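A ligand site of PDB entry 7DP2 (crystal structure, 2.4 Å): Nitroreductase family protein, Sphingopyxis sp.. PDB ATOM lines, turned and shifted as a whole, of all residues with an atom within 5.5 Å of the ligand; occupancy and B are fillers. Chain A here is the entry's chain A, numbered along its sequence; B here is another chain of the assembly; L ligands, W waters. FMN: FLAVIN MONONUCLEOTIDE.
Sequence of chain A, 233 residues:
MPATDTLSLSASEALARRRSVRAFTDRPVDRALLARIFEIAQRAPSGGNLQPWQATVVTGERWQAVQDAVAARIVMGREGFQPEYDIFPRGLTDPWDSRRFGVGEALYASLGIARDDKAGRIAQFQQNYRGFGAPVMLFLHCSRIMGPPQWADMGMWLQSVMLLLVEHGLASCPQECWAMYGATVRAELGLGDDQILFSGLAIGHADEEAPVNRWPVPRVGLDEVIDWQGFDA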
ATOM      1  N   ARG A  18       6.314 -26.159 -27.287  1.00  0.00           N
ATOM      2  CA  ARG A  18       6.710 -24.761 -27.319  1.00  0.00           C
ATOM      3  C   ARG A  18       7.528 -24.410 -26.083  1.00  0.00           C
ATOM      4  O   ARG A  18       7.111 -24.697 -24.968  1.00  0.00           O
ATOM      5  CB  ARG A  18       5.506 -23.825 -27.414  1.00  0.00           C
ATOM      6  CG  ARG A  18       5.916 -22.379 -27.586  1.00  0.00           C
ATOM      7  CD  ARG A  18       5.078 -21.445 -26.728  1.00  0.00           C
ATOM      8  NE  ARG A  18       5.130 -21.807 -25.320  1.00  0.00           N
ATOM      9  CZ  ARG A  18       6.122 -21.515 -24.478  1.00  0.00           C
ATOM     10  NH1 ARG A  18       7.204 -20.842 -24.894  1.00  0.00           N
ATOM     11  NH2 ARG A  18       6.037 -21.909 -23.213  1.00  0.00           N
ATOM     12  N   ARG A  19       8.705 -23.824 -26.300  1.00  0.00           N
ATOM     13  CA  ARG A  19       9.476 -23.201 -25.226  1.00  0.00           C
ATOM     14  C   ARG A  19      10.134 -21.917 -25.724  1.00  0.00           C
ATOM     15  O   ARG A  19      10.261 -21.678 -26.931  1.00  0.00           O
ATOM     16  CB  ARG A  19      10.532 -24.136 -24.688  1.00  0.00           C
ATOM     17  CG  ARG A  19      11.664 -24.336 -25.655  1.00  0.00           C
ATOM     18  CD  ARG A  19      12.687 -25.316 -25.111  1.00  0.00           C
ATOM     19  NE  ARG A  19      13.447 -24.784 -23.986  1.00  0.00           N
ATOM     20  CZ  ARG A  19      13.903 -25.530 -22.979  1.00  0.00           C
ATOM     21  NH1 ARG A  19      13.671 -26.843 -22.961  1.00  0.00           N
ATOM     22  NH2 ARG A  19      14.591 -24.961 -21.988  1.00  0.00           N
ATOM     23  N   SER A  20      10.551 -21.087 -24.784  1.00  0.00           N
ATOM     24  CA  SER A  20      11.327 -19.926 -25.183  1.00  0.00           C
ATOM     25  C   SER A  20      12.704 -20.405 -25.629  1.00  0.00           C
ATOM     26  O   SER A  20      13.470 -20.916 -24.818  1.00  0.00           O
ATOM     27  CB  SER A  20      11.432 -18.935 -24.047  1.00  0.00           C
ATOM     28  OG  SER A  20      10.136 -18.649 -23.575  1.00  0.00           O
ATOM     29  N   VAL A  21      12.990 -20.288 -26.923  1.00  0.00           N
ATOM     30  CA  VAL A  21      14.234 -20.788 -27.491  1.00  0.00           C
ATOM     31  C   VAL A  21      15.321 -19.704 -27.553  1.00  0.00           C
ATOM     32  O   VAL A  21      15.087 -18.608 -28.063  1.00  0.00           O
ATOM     33  CB  VAL A  21      13.995 -21.355 -28.893  1.00  0.00           C
ATOM     34  CG1 VAL A  21      15.306 -21.547 -29.627  1.00  0.00           C
ATOM     35  CG2 VAL A  21      13.252 -22.692 -28.770  1.00  0.00           C
ATOM     36  N   ARG A  22      16.503 -19.999 -27.030  1.00  0.00           N
ATOM     37  CA  ARG A  22      17.543 -18.968 -26.944  1.00  0.00           C
ATOM     38  C   ARG A  22      18.796 -19.314 -27.712  1.00  0.00           C
ATOM     39  O   ARG A  22      19.911 -18.936 -27.318  1.00  0.00           O
ATOM     40  CB  ARG A  22      17.876 -18.691 -25.472  1.00  0.00           C
ATOM     41  CG  ARG A  22      16.812 -17.843 -24.818  1.00  0.00           C
ATOM     42  CD  ARG A  22      16.734 -18.065 -23.338  1.00  0.00           C
ATOM     43  NE  ARG A  22      15.588 -17.349 -22.779  1.00  0.00           N
ATOM     44  CZ  ARG A  22      14.627 -17.919 -22.067  1.00  0.00           C
ATOM     45  NH1 ARG A  22      14.660 -19.225 -21.829  1.00  0.00           N
ATOM     46  NH2 ARG A  22      13.622 -17.192 -21.592  1.00  0.00           N
ATOM     47  N   VAL A 103      13.569 -19.888 -12.777  1.00  0.00           N
ATOM     48  CA  VAL A 103      13.880 -20.337 -14.132  1.00  0.00           C
ATOM     49  C   VAL A 103      15.224 -19.771 -14.542  1.00  0.00           C
ATOM     50  O   VAL A 103      15.944 -20.391 -15.324  1.00  0.00           O
ATOM     51  CB  VAL A 103      12.808 -19.919 -15.135  1.00  0.00           C
ATOM     52  CG1 VAL A 103      11.484 -20.609 -14.822  1.00  0.00           C
ATOM     53  CG2 VAL A 103      12.639 -18.405 -15.159  1.00  0.00           C
ATOM     54  N   PHE A 125      22.741 -12.405 -20.996  1.00  0.00           N
ATOM     55  CA  PHE A 125      21.525 -11.602 -21.093  1.00  0.00           C
ATOM     56  C   PHE A 125      21.499 -10.647 -22.262  1.00  0.00           C
ATOM     57  O   PHE A 125      20.489 -10.514 -22.940  1.00  0.00           O
ATOM     58  CB  PHE A 125      21.291 -10.775 -19.816  1.00  0.00           C
ATOM     59  CG  PHE A 125      20.009  -9.981 -19.847  1.00  0.00           C
ATOM     60  CD1 PHE A 125      18.779 -10.585 -19.640  1.00  0.00           C
ATOM     61  CD2 PHE A 125      20.029  -8.615 -20.125  1.00  0.00           C
ATOM     62  CE1 PHE A 125      17.589  -9.840 -19.688  1.00  0.00           C
ATOM     63  CE2 PHE A 125      18.839  -7.870 -20.172  1.00  0.00           C
ATOM     64  CZ  PHE A 125      17.626  -8.490 -19.956  1.00  0.00           C
ATOM     65  N   ASN A 128      19.920 -11.179 -25.635  1.00  0.00           N
ATOM     66  CA  ASN A 128      18.507 -10.832 -25.832  1.00  0.00           C
ATOM     67  C   ASN A 128      18.377  -9.891 -26.990  1.00  0.00           C
ATOM     68  O   ASN A 128      17.476 -10.006 -27.820  1.00  0.00           O
ATOM     69  CB  ASN A 128      17.915 -10.173 -24.577  1.00  0.00           C
ATOM     70  CG  ASN A 128      17.236 -11.157 -23.656  1.00  0.00           C
ATOM     71  OD1 ASN A 128      16.093 -11.550 -23.870  1.00  0.00           O
ATOM     72  ND2 ASN A 128      17.961 -11.569 -22.621  1.00  0.00           N
ATOM     73  N   PHE A 132      18.722 -13.410 -29.783  1.00  0.00           N
ATOM     74  CA  PHE A 132      19.386 -14.694 -29.651  1.00  0.00           C
ATOM     75  C   PHE A 132      19.796 -15.264 -30.990  1.00  0.00           C
ATOM     76  O   PHE A 132      19.932 -16.473 -31.151  1.00  0.00           O
ATOM     77  CB  PHE A 132      18.477 -15.681 -28.893  1.00  0.00           C
ATOM     78  CG  PHE A 132      18.096 -15.217 -27.521  1.00  0.00           C
ATOM     79  CD1 PHE A 132      19.084 -15.076 -26.537  1.00  0.00           C
ATOM     80  CD2 PHE A 132      16.781 -14.912 -27.197  1.00  0.00           C
ATOM     81  CE1 PHE A 132      18.756 -14.648 -25.266  1.00  0.00           C
ATOM     82  CE2 PHE A 132      16.450 -14.477 -25.911  1.00  0.00           C
ATOM     83  CZ  PHE A 132      17.434 -14.348 -24.948  1.00  0.00           C
ATOM     84  N   LEU A 158      -0.610 -13.755 -29.567  1.00  0.00           N
ATOM     85  CA  LEU A 158       0.794 -14.090 -29.506  1.00  0.00           C
ATOM     86  C   LEU A 158       0.982 -15.599 -29.268  1.00  0.00           C
ATOM     87  O   LEU A 158       1.742 -16.255 -29.981  1.00  0.00           O
ATOM     88  CB  LEU A 158       1.490 -13.268 -28.400  1.00  0.00           C
ATOM     89  CG  LEU A 158       3.016 -13.389 -28.476  1.00  0.00           C
ATOM     90  CD1 LEU A 158       3.519 -12.899 -29.816  1.00  0.00           C
ATOM     91  CD2 LEU A 158       3.705 -12.647 -27.350  1.00  0.00           C
ATOM     92  N   CYS A 173      11.101 -16.922 -29.331  1.00  0.00           N
ATOM     93  CA  CYS A 173      11.303 -16.472 -27.982  1.00  0.00           C
ATOM     94  C   CYS A 173      10.598 -15.133 -27.768  1.00  0.00           C
ATOM     95  O   CYS A 173      10.913 -14.147 -28.428  1.00  0.00           O
ATOM     96  CB  CYS A 173      12.796 -16.351 -27.665  1.00  0.00           C
ATOM     97  SG  CYS A 173      13.087 -15.919 -25.923  1.00  0.00           S
ATOM     98  N   PRO A 174       9.604 -15.116 -26.884  1.00  0.00           N
ATOM     99  CA  PRO A 174       8.981 -13.839 -26.509  1.00  0.00           C
ATOM    100  C   PRO A 174       9.983 -12.973 -25.736  1.00  0.00           C
ATOM    101  O   PRO A 174      10.752 -13.479 -24.933  1.00  0.00           O
ATOM    102  CB  PRO A 174       7.801 -14.243 -25.609  1.00  0.00           C
ATOM    103  CG  PRO A 174       7.697 -15.756 -25.702  1.00  0.00           C
ATOM    104  CD  PRO A 174       9.034 -16.268 -26.162  1.00  0.00           C
ATOM    105  N   GLN A 175       9.980 -11.668 -26.025  1.00  0.00           N
ATOM    106  CA  GLN A 175      10.943 -10.749 -25.438  1.00  0.00           C
ATOM    107  C   GLN A 175      10.327  -9.414 -25.049  1.00  0.00           C
ATOM    108  O   GLN A 175      10.048  -8.585 -25.914  1.00  0.00           O
ATOM    109  CB  GLN A 175      12.082 -10.502 -26.406  1.00  0.00           C
ATOM    110  CG  GLN A 175      12.936 -11.690 -26.687  1.00  0.00           C
ATOM    111  CD  GLN A 175      14.189 -11.298 -27.386  1.00  0.00           C
ATOM    112  OE1 GLN A 175      14.177 -10.930 -28.571  1.00  0.00           O
ATOM    113  NE2 GLN A 175      15.302 -11.358 -26.679  1.00  0.00           N
ATOM    114  N   GLU A 176      10.167  -9.197 -23.752  1.00  0.00           N
ATOM    115  CA  GLU A 176       9.734  -7.909 -23.226  1.00  0.00           C
ATOM    116  C   GLU A 176      10.912  -6.948 -23.125  1.00  0.00           C
ATOM    117  O   GLU A 176      10.732  -5.763 -22.859  1.00  0.00           O
ATOM    118  CB  GLU A 176       9.097  -8.076 -21.851  1.00  0.00           C
ATOM    119  CG  GLU A 176       7.615  -8.278 -21.861  1.00  0.00           C
ATOM    120  CD  GLU A 176       7.110  -9.029 -20.640  1.00  0.00           C
ATOM    121  OE1 GLU A 176       7.922  -9.526 -19.825  1.00  0.00           O
ATOM    122  OE2 GLU A 176       5.881  -9.151 -20.489  1.00  0.00           O
ATOM    123  N   CYS A 177      12.112  -7.469 -23.334  1.00  0.00           N
ATOM    124  CA  CYS A 177      13.318  -6.694 -23.100  1.00  0.00           C
ATOM    125  C   CYS A 177      13.380  -5.452 -23.996  1.00  0.00           C
ATOM    126  O   CYS A 177      13.901  -4.410 -23.582  1.00  0.00           O
ATOM    127  CB  CYS A 177      14.564  -7.584 -23.311  1.00  0.00           C
ATOM    128  SG  CYS A 177      14.710  -8.340 -24.972  1.00  0.00           S
ATOM    129  N   PHE A 198       4.599  -3.519 -27.059  1.00  0.00           N
ATOM    130  CA  PHE A 198       4.363  -4.480 -25.996  1.00  0.00           C
ATOM    131  C   PHE A 198       5.584  -5.378 -25.882  1.00  0.00           C
ATOM    132  O   PHE A 198       6.277  -5.388 -24.869  1.00  0.00           O
ATOM    133  CB  PHE A 198       3.089  -5.312 -26.245  1.00  0.00           C
ATOM    134  CG  PHE A 198       3.037  -6.611 -25.470  1.00  0.00           C
ATOM    135  CD1 PHE A 198       3.395  -6.677 -24.132  1.00  0.00           C
ATOM    136  CD2 PHE A 198       2.606  -7.769 -26.083  1.00  0.00           C
ATOM    137  CE1 PHE A 198       3.348  -7.871 -23.427  1.00  0.00           C
ATOM    138  CE2 PHE A 198       2.555  -8.980 -25.378  1.00  0.00           C
ATOM    139  CZ  PHE A 198       2.910  -9.016 -24.060  1.00  0.00           C
ATOM    140  N   SER A 199       5.848  -6.126 -26.930  1.00  0.00           N
ATOM    141  CA  SER A 199       6.834  -7.182 -26.816  1.00  0.00           C
ATOM    142  C   SER A 199       7.434  -7.467 -28.169  1.00  0.00           C
ATOM    143  O   SER A 199       6.854  -7.091 -29.189  1.00  0.00           O
ATOM    144  CB  SER A 199       6.174  -8.435 -26.236  1.00  0.00           C
ATOM    145  OG  SER A 199       7.053  -9.529 -26.193  1.00  0.00           O
ATOM    146  N   TRP A 215      17.096 -27.796 -21.337  1.00  0.00           N
ATOM    147  CA  TRP A 215      16.875 -27.971 -19.901  1.00  0.00           C
ATOM    148  C   TRP A 215      15.384 -27.955 -19.611  1.00  0.00           C
ATOM    149  O   TRP A 215      14.637 -27.209 -20.251  1.00  0.00           O
ATOM    150  CB  TRP A 215      17.629 -26.894 -19.113  1.00  0.00           C
ATOM    151  CG  TRP A 215      17.267 -25.529 -19.569  1.00  0.00           C
ATOM    152  CD1 TRP A 215      17.804 -24.848 -20.619  1.00  0.00           C
ATOM    153  CD2 TRP A 215      16.276 -24.663 -18.997  1.00  0.00           C
ATOM    154  NE1 TRP A 215      17.196 -23.622 -20.752  1.00  0.00           N
ATOM    155  CE2 TRP A 215      16.256 -23.485 -19.767  1.00  0.00           C
ATOM    156  CE3 TRP A 215      15.394 -24.772 -17.918  1.00  0.00           C
ATOM    157  CZ2 TRP A 215      15.402 -22.421 -19.490  1.00  0.00           C
ATOM    158  CZ3 TRP A 215      14.533 -23.712 -17.648  1.00  0.00           C
ATOM    159  CH2 TRP A 215      14.550 -22.554 -18.426  1.00  0.00           C
ATOM    160  N   VAL A 217      11.915 -27.015 -18.330  1.00  0.00           N
ATOM    161  CA  VAL A 217      11.404 -25.764 -17.773  1.00  0.00           C
ATOM    162  C   VAL A 217      10.334 -26.030 -16.749  1.00  0.00           C
ATOM    163  O   VAL A 217       9.362 -26.718 -17.028  1.00  0.00           O
ATOM    164  CB  VAL A 217      10.843 -24.845 -18.866  1.00  0.00           C
ATOM    165  CG1 VAL A 217      10.501 -23.429 -18.306  1.00  0.00           C
ATOM    166  CG2 VAL A 217      11.819 -24.768 -20.027  1.00  0.00           C
ATOM    167  N   ARG A 219       7.159 -25.504 -14.178  1.00  0.00           N
ATOM    168  CA  ARG A 219       5.901 -24.817 -13.964  1.00  0.00           C
ATOM    169  C   ARG A 219       5.446 -25.157 -12.558  1.00  0.00           C
ATOM    170  O   ARG A 219       5.841 -26.192 -12.040  1.00  0.00           O
ATOM    171  CB  ARG A 219       4.844 -25.246 -14.985  1.00  0.00           C
ATOM    172  CG  ARG A 219       5.031 -24.739 -16.386  1.00  0.00           C
ATOM    173  CD  ARG A 219       5.082 -23.241 -16.427  1.00  0.00           C
ATOM    174  NE  ARG A 219       5.018 -22.735 -17.798  1.00  0.00           N
ATOM    175  CZ  ARG A 219       6.062 -22.667 -18.619  1.00  0.00           C
ATOM    176  NH1 ARG A 219       7.250 -23.076 -18.218  1.00  0.00           N
ATOM    177  NH2 ARG A 219       5.905 -22.199 -19.853  1.00  0.00           N
ATOM    178  N   ARG B  43       1.693 -25.009 -19.390  1.00  0.00           N
ATOM    179  CA  ARG B  43       2.895 -24.844 -20.194  1.00  0.00           C
ATOM    180  C   ARG B  43       2.890 -23.546 -21.006  1.00  0.00           C
ATOM    181  O   ARG B  43       3.819 -23.306 -21.779  1.00  0.00           O
ATOM    182  CB  ARG B  43       3.088 -26.024 -21.146  1.00  0.00           C
ATOM    183  CG  ARG B  43       3.106 -27.349 -20.447  1.00  0.00           C
ATOM    184  CD  ARG B  43       4.018 -27.372 -19.247  1.00  0.00           C
ATOM    185  NE  ARG B  43       5.421 -27.106 -19.557  1.00  0.00           N
ATOM    186  CZ  ARG B  43       6.400 -27.235 -18.675  1.00  0.00           C
ATOM    187  NH1 ARG B  43       6.132 -27.639 -17.432  1.00  0.00           N
ATOM    188  NH2 ARG B  43       7.651 -26.961 -19.022  1.00  0.00           N
ATOM    189  N   ALA B  44       1.837 -22.744 -20.895  1.00  0.00           N
ATOM    190  CA  ALA B  44       1.815 -21.446 -21.551  1.00  0.00           C
ATOM    191  C   ALA B  44       2.974 -20.586 -21.005  1.00  0.00           C
ATOM    192  O   ALA B  44       3.371 -20.746 -19.861  1.00  0.00           O
ATOM    193  CB  ALA B  44       0.444 -20.749 -21.353  1.00  0.00           C
ATOM    194  N   PRO B  45       3.539 -19.701 -21.836  1.00  0.00           N
ATOM    195  CA  PRO B  45       4.632 -18.840 -21.369  1.00  0.00           C
ATOM    196  C   PRO B  45       4.136 -17.641 -20.547  1.00  0.00           C
ATOM    197  O   PRO B  45       2.939 -17.336 -20.513  1.00  0.00           O
ATOM    198  CB  PRO B  45       5.294 -18.382 -22.660  1.00  0.00           C
ATOM    199  CG  PRO B  45       4.155 -18.357 -23.653  1.00  0.00           C
ATOM    200  CD  PRO B  45       3.223 -19.492 -23.266  1.00  0.00           C
ATOM    201  N   SER B  46       5.060 -16.990 -19.858  1.00  0.00           N
ATOM    202  CA  SER B  46       4.732 -15.763 -19.148  1.00  0.00           C
ATOM    203  C   SER B  46       6.038 -15.026 -18.947  1.00  0.00           C
ATOM    204  O   SER B  46       7.078 -15.644 -18.743  1.00  0.00           O
ATOM    205  CB  SER B  46       4.030 -16.059 -17.820  1.00  0.00           C
ATOM    206  OG  SER B  46       4.721 -17.081 -17.104  1.00  0.00           O
ATOM    207  N   GLY B  47       5.987 -13.697 -19.064  1.00  0.00           N
ATOM    208  CA  GLY B  47       7.151 -12.878 -18.833  1.00  0.00           C
ATOM    209  C   GLY B  47       7.725 -13.295 -17.500  1.00  0.00           C
ATOM    210  O   GLY B  47       7.004 -13.374 -16.509  1.00  0.00           O
ATOM    211  N   GLY B  48       9.002 -13.605 -17.502  1.00  0.00           N
ATOM    212  CA  GLY B  48       9.683 -14.070 -16.306  1.00  0.00           C
ATOM    213  C   GLY B  48       9.116 -15.353 -15.706  1.00  0.00           C
ATOM    214  O   GLY B  48       9.442 -15.669 -14.580  1.00  0.00           O
ATOM    215  N   ASN B  49       8.275 -16.099 -16.433  1.00  0.00           N
ATOM    216  CA  ASN B  49       7.559 -17.222 -15.857  1.00  0.00           C
ATOM    217  C   ASN B  49       6.900 -16.931 -14.527  1.00  0.00           C
ATOM    218  O   ASN B  49       7.106 -17.661 -13.553  1.00  0.00           O
ATOM    219  CB  ASN B  49       8.467 -18.452 -15.825  1.00  0.00           C
ATOM    220  CG  ASN B  49       7.681 -19.762 -15.690  1.00  0.00           C
ATOM    221  OD1 ASN B  49       6.592 -19.771 -15.104  1.00  0.00           O
ATOM    222  ND2 ASN B  49       8.131 -20.831 -16.372  1.00  0.00           N
ATOM    223  N   PRO B 149       1.349  -6.210 -18.988  1.00  0.00           N
ATOM    224  CA  PRO B 149       2.074  -7.381 -19.528  1.00  0.00           C
ATOM    225  C   PRO B 149       1.603  -8.713 -18.931  1.00  0.00           C
ATOM    226  O   PRO B 149       1.470  -9.705 -19.675  1.00  0.00           O
ATOM    227  CB  PRO B 149       3.542  -7.105 -19.149  1.00  0.00           C
ATOM    228  CG  PRO B 149       3.466  -6.136 -18.028  1.00  0.00           C
ATOM    229  CD  PRO B 149       2.296  -5.263 -18.352  1.00  0.00           C
ATOM    230  N   ASP B 153      -0.038 -12.222 -20.348  1.00  0.00           N
ATOM    231  CA  ASP B 153       0.268 -13.599 -19.887  1.00  0.00           C
ATOM    232  C   ASP B 153      -1.011 -14.430 -19.720  1.00  0.00           C
ATOM    233  O   ASP B 153      -1.073 -15.562 -20.195  1.00  0.00           O
ATOM    234  CB  ASP B 153       0.989 -13.610 -18.546  1.00  0.00           C
ATOM    235  CG  ASP B 153       2.342 -12.940 -18.569  1.00  0.00           C
ATOM    236  OD1 ASP B 153       2.990 -12.894 -19.638  1.00  0.00           O
ATOM    237  OD2 ASP B 153       2.752 -12.454 -17.486  1.00  0.00           O
ATOM    238  N   MET B 156      -2.429 -15.575 -22.861  1.00  0.00           N
ATOM    239  CA  MET B 156      -1.708 -16.739 -23.386  1.00  0.00           C
ATOM    240  C   MET B 156      -2.186 -18.047 -22.750  1.00  0.00           C
ATOM    241  O   MET B 156      -2.353 -19.048 -23.414  1.00  0.00           O
ATOM    242  CB  MET B 156      -0.224 -16.576 -23.159  1.00  0.00           C
ATOM    243  CG  MET B 156       0.346 -15.437 -23.940  1.00  0.00           C
ATOM    244  SD  MET B 156       1.985 -15.011 -23.326  1.00  0.00           S
ATOM    245  CE  MET B 156       2.119 -13.314 -23.911  1.00  0.00           C
HETATM  246  N1  FMN L   1      12.698 -14.546 -22.124  1.00  0.00           N
HETATM  247  C2  FMN L   1      13.882 -13.854 -22.244  1.00  0.00           C
HETATM  248  O2  FMN L   1      14.942 -14.466 -22.155  1.00  0.00           O
HETATM  249  N3  FMN L   1      13.898 -12.498 -22.442  1.00  0.00           N
HETATM  250  C4  FMN L   1      12.729 -11.793 -22.532  1.00  0.00           C
HETATM  251  O4  FMN L   1      12.714 -10.567 -22.711  1.00  0.00           O
HETATM  252  C4A FMN L   1      11.535 -12.483 -22.402  1.00  0.00           C
HETATM  253  N5  FMN L   1      10.365 -11.795 -22.478  1.00  0.00           N
HETATM  254  C5A FMN L   1       9.165 -12.455 -22.382  1.00  0.00           C
HETATM  255  C6  FMN L   1       8.006 -11.705 -22.502  1.00  0.00           C
HETATM  256  C7  FMN L   1       6.780 -12.318 -22.412  1.00  0.00           C
HETATM  257  C7M FMN L   1       5.517 -11.511 -22.528  1.00  0.00           C
HETATM  258  C8  FMN L   1       6.716 -13.687 -22.219  1.00  0.00           C
HETATM  259  C8M FMN L   1       5.363 -14.333 -22.130  1.00  0.00           C
HETATM  260  C9  FMN L   1       7.882 -14.444 -22.101  1.00  0.00           C
HETATM  261  C9A FMN L   1       9.135 -13.837 -22.182  1.00  0.00           C
HETATM  262  N10 FMN L   1      10.338 -14.543 -22.078  1.00  0.00           N
HETATM  263  C10 FMN L   1      11.518 -13.856 -22.191  1.00  0.00           C
HETATM  264  C1' FMN L   1      10.430 -16.021 -21.875  1.00  0.00           C
HETATM  265  C2' FMN L   1       9.927 -16.480 -20.491  1.00  0.00           C
HETATM  266  O2' FMN L   1      10.904 -16.442 -19.464  1.00  0.00           O
HETATM  267  C3' FMN L   1       9.384 -17.903 -20.614  1.00  0.00           C
HETATM  268  O3' FMN L   1       8.138 -17.815 -21.259  1.00  0.00           O
HETATM  269  C4' FMN L   1       9.166 -18.599 -19.284  1.00  0.00           C
HETATM  270  O4' FMN L   1      10.333 -18.592 -18.486  1.00  0.00           O
HETATM  271  C5' FMN L   1       8.747 -20.032 -19.524  1.00  0.00           C
HETATM  272  O5' FMN L   1       9.790 -20.733 -20.183  1.00  0.00           O
HETATM  273  P   FMN L   1       9.375 -21.435 -21.570  1.00  0.00           P
HETATM  274  O1P FMN L   1       8.470 -22.600 -21.292  1.00  0.00           O
HETATM  275  O2P FMN L   1       8.591 -20.430 -22.337  1.00  0.00           O
HETATM  276  O3P FMN L   1      10.615 -21.807 -22.336  1.00  0.00           O
HETATM  277  O   HOH W   1      11.498 -13.274 -18.995  1.00  0.00           O
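N1 of the ligand sits at hydrogen-bond distance from NH2 of Arg 22, 2.9 Å away.
A nitrogen (N3) of the ligand lies within hydrogen-bond range of the side-chain amide oxygen (OD1) of Asn 128.
O1P of the ligand lies within salt-bridge range of NH2 of Arg 219 (3.0 Å).
The guanidinium group of Arg 18 is in salt-bridge range of an oxygen (O2P) of the ligand (2.9 Å).
O3' of the ligand lies close to O of Ser 46 of chain B, at 3.5 Å.
N of Ser 46 of chain B lies within hydrogen-bond range of O3' of the ligand (3.5 Å).
The backbone NH (N) of Ser 20 is in hydrogen-bond range of an oxygen (O3P) of the ligand, 2.6 Å away.
OG of Ser 20 lies within hydrogen-bond range of O2P of the ligand, 2.7 Å away.
N of Cys 177 is in hydrogen-bond range of O4 of the ligand, 3.2 Å away.
An oxygen (O4) of the ligand sits close to the side-chain sulfur (SG) of Cys 177, 3.7 Å away.
N of Glu 176 sits at hydrogen-bond distance from N5 of the ligand (2.9 Å).
Water W1 bridges the backbone NH (N) of Gly 48 of chain B (2.9 Å) and an oxygen (O2') of the ligand (3.3 Å).
O of Pro 174 lies close to N5 of the ligand (3.0 Å).
Arg 19 touches the ligand (CB to O3P, 3.3 Å).
Phe 132 touches the ligand.
CA of Gln 175 touches N5 of the ligand, 3.2 Å away.
CZ of Phe 198 touches C7M of the ligand (3.9 Å).
Val 217 touches the ligand (CG1 to O5', 3.4 Å).
CB of Pro 45 of chain B touches O3' of the ligand (3.2 Å).
Gly 47 of chain B touches the ligand.
Gly 48 of chain B touches the ligand (N to O2', 3.9 Å).
CB of Asn 49 of chain B touches O4' of the ligand (3.3 Å).
Asp 153 of chain B touches the ligand.
SD of Met 156 of chain B touches C8M of the ligand, 3.6 Å away.
Hydrophobic or aromatic side chains that line the ligand: Phe 132, Pro 174, Phe 198, Val 217, Pro 45 of chain B and Met 156 of chain B.
The nearest printed residue that does not touch the ligand is Val 103 (4.1 Å).
The backbone NH (N) of Gly 47 of chain B sits at hydrogen-bond distance from the side-chain carboxylate (OD1) of Asp 153 of chain B (3.2 Å).
The side-chain amide nitrogen (NE2) of Gln 175 is in hydrogen-bond range of the side-chain sulfur (SG) of Cys 177, 3.5 Å away.
OD1 of Asn 128 is in hydrogen-bond range of SG of Cys 177, 3.7 Å away.
O of Val 217 sits at hydrogen-bond distance from NH2 of Arg 43 of chain B.
NH2 of Arg 219 sits at hydrogen-bond distance from O of Arg 43 of chain B (3.0 Å).
The guanidinium group of Arg 219 sits at hydrogen-bond distance from the backbone carbonyl oxygen of Ala 44 of chain B.
The backbone carbonyl oxygen of Arg 43 of chain B is in hydrogen-bond range of the guanidinium group of Arg 18.
The backbone carbonyl oxygen (O) of Gln 175 sits at hydrogen-bond distance from the side-chain hydroxyl (OG) of Ser 199 (3.2 Å).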
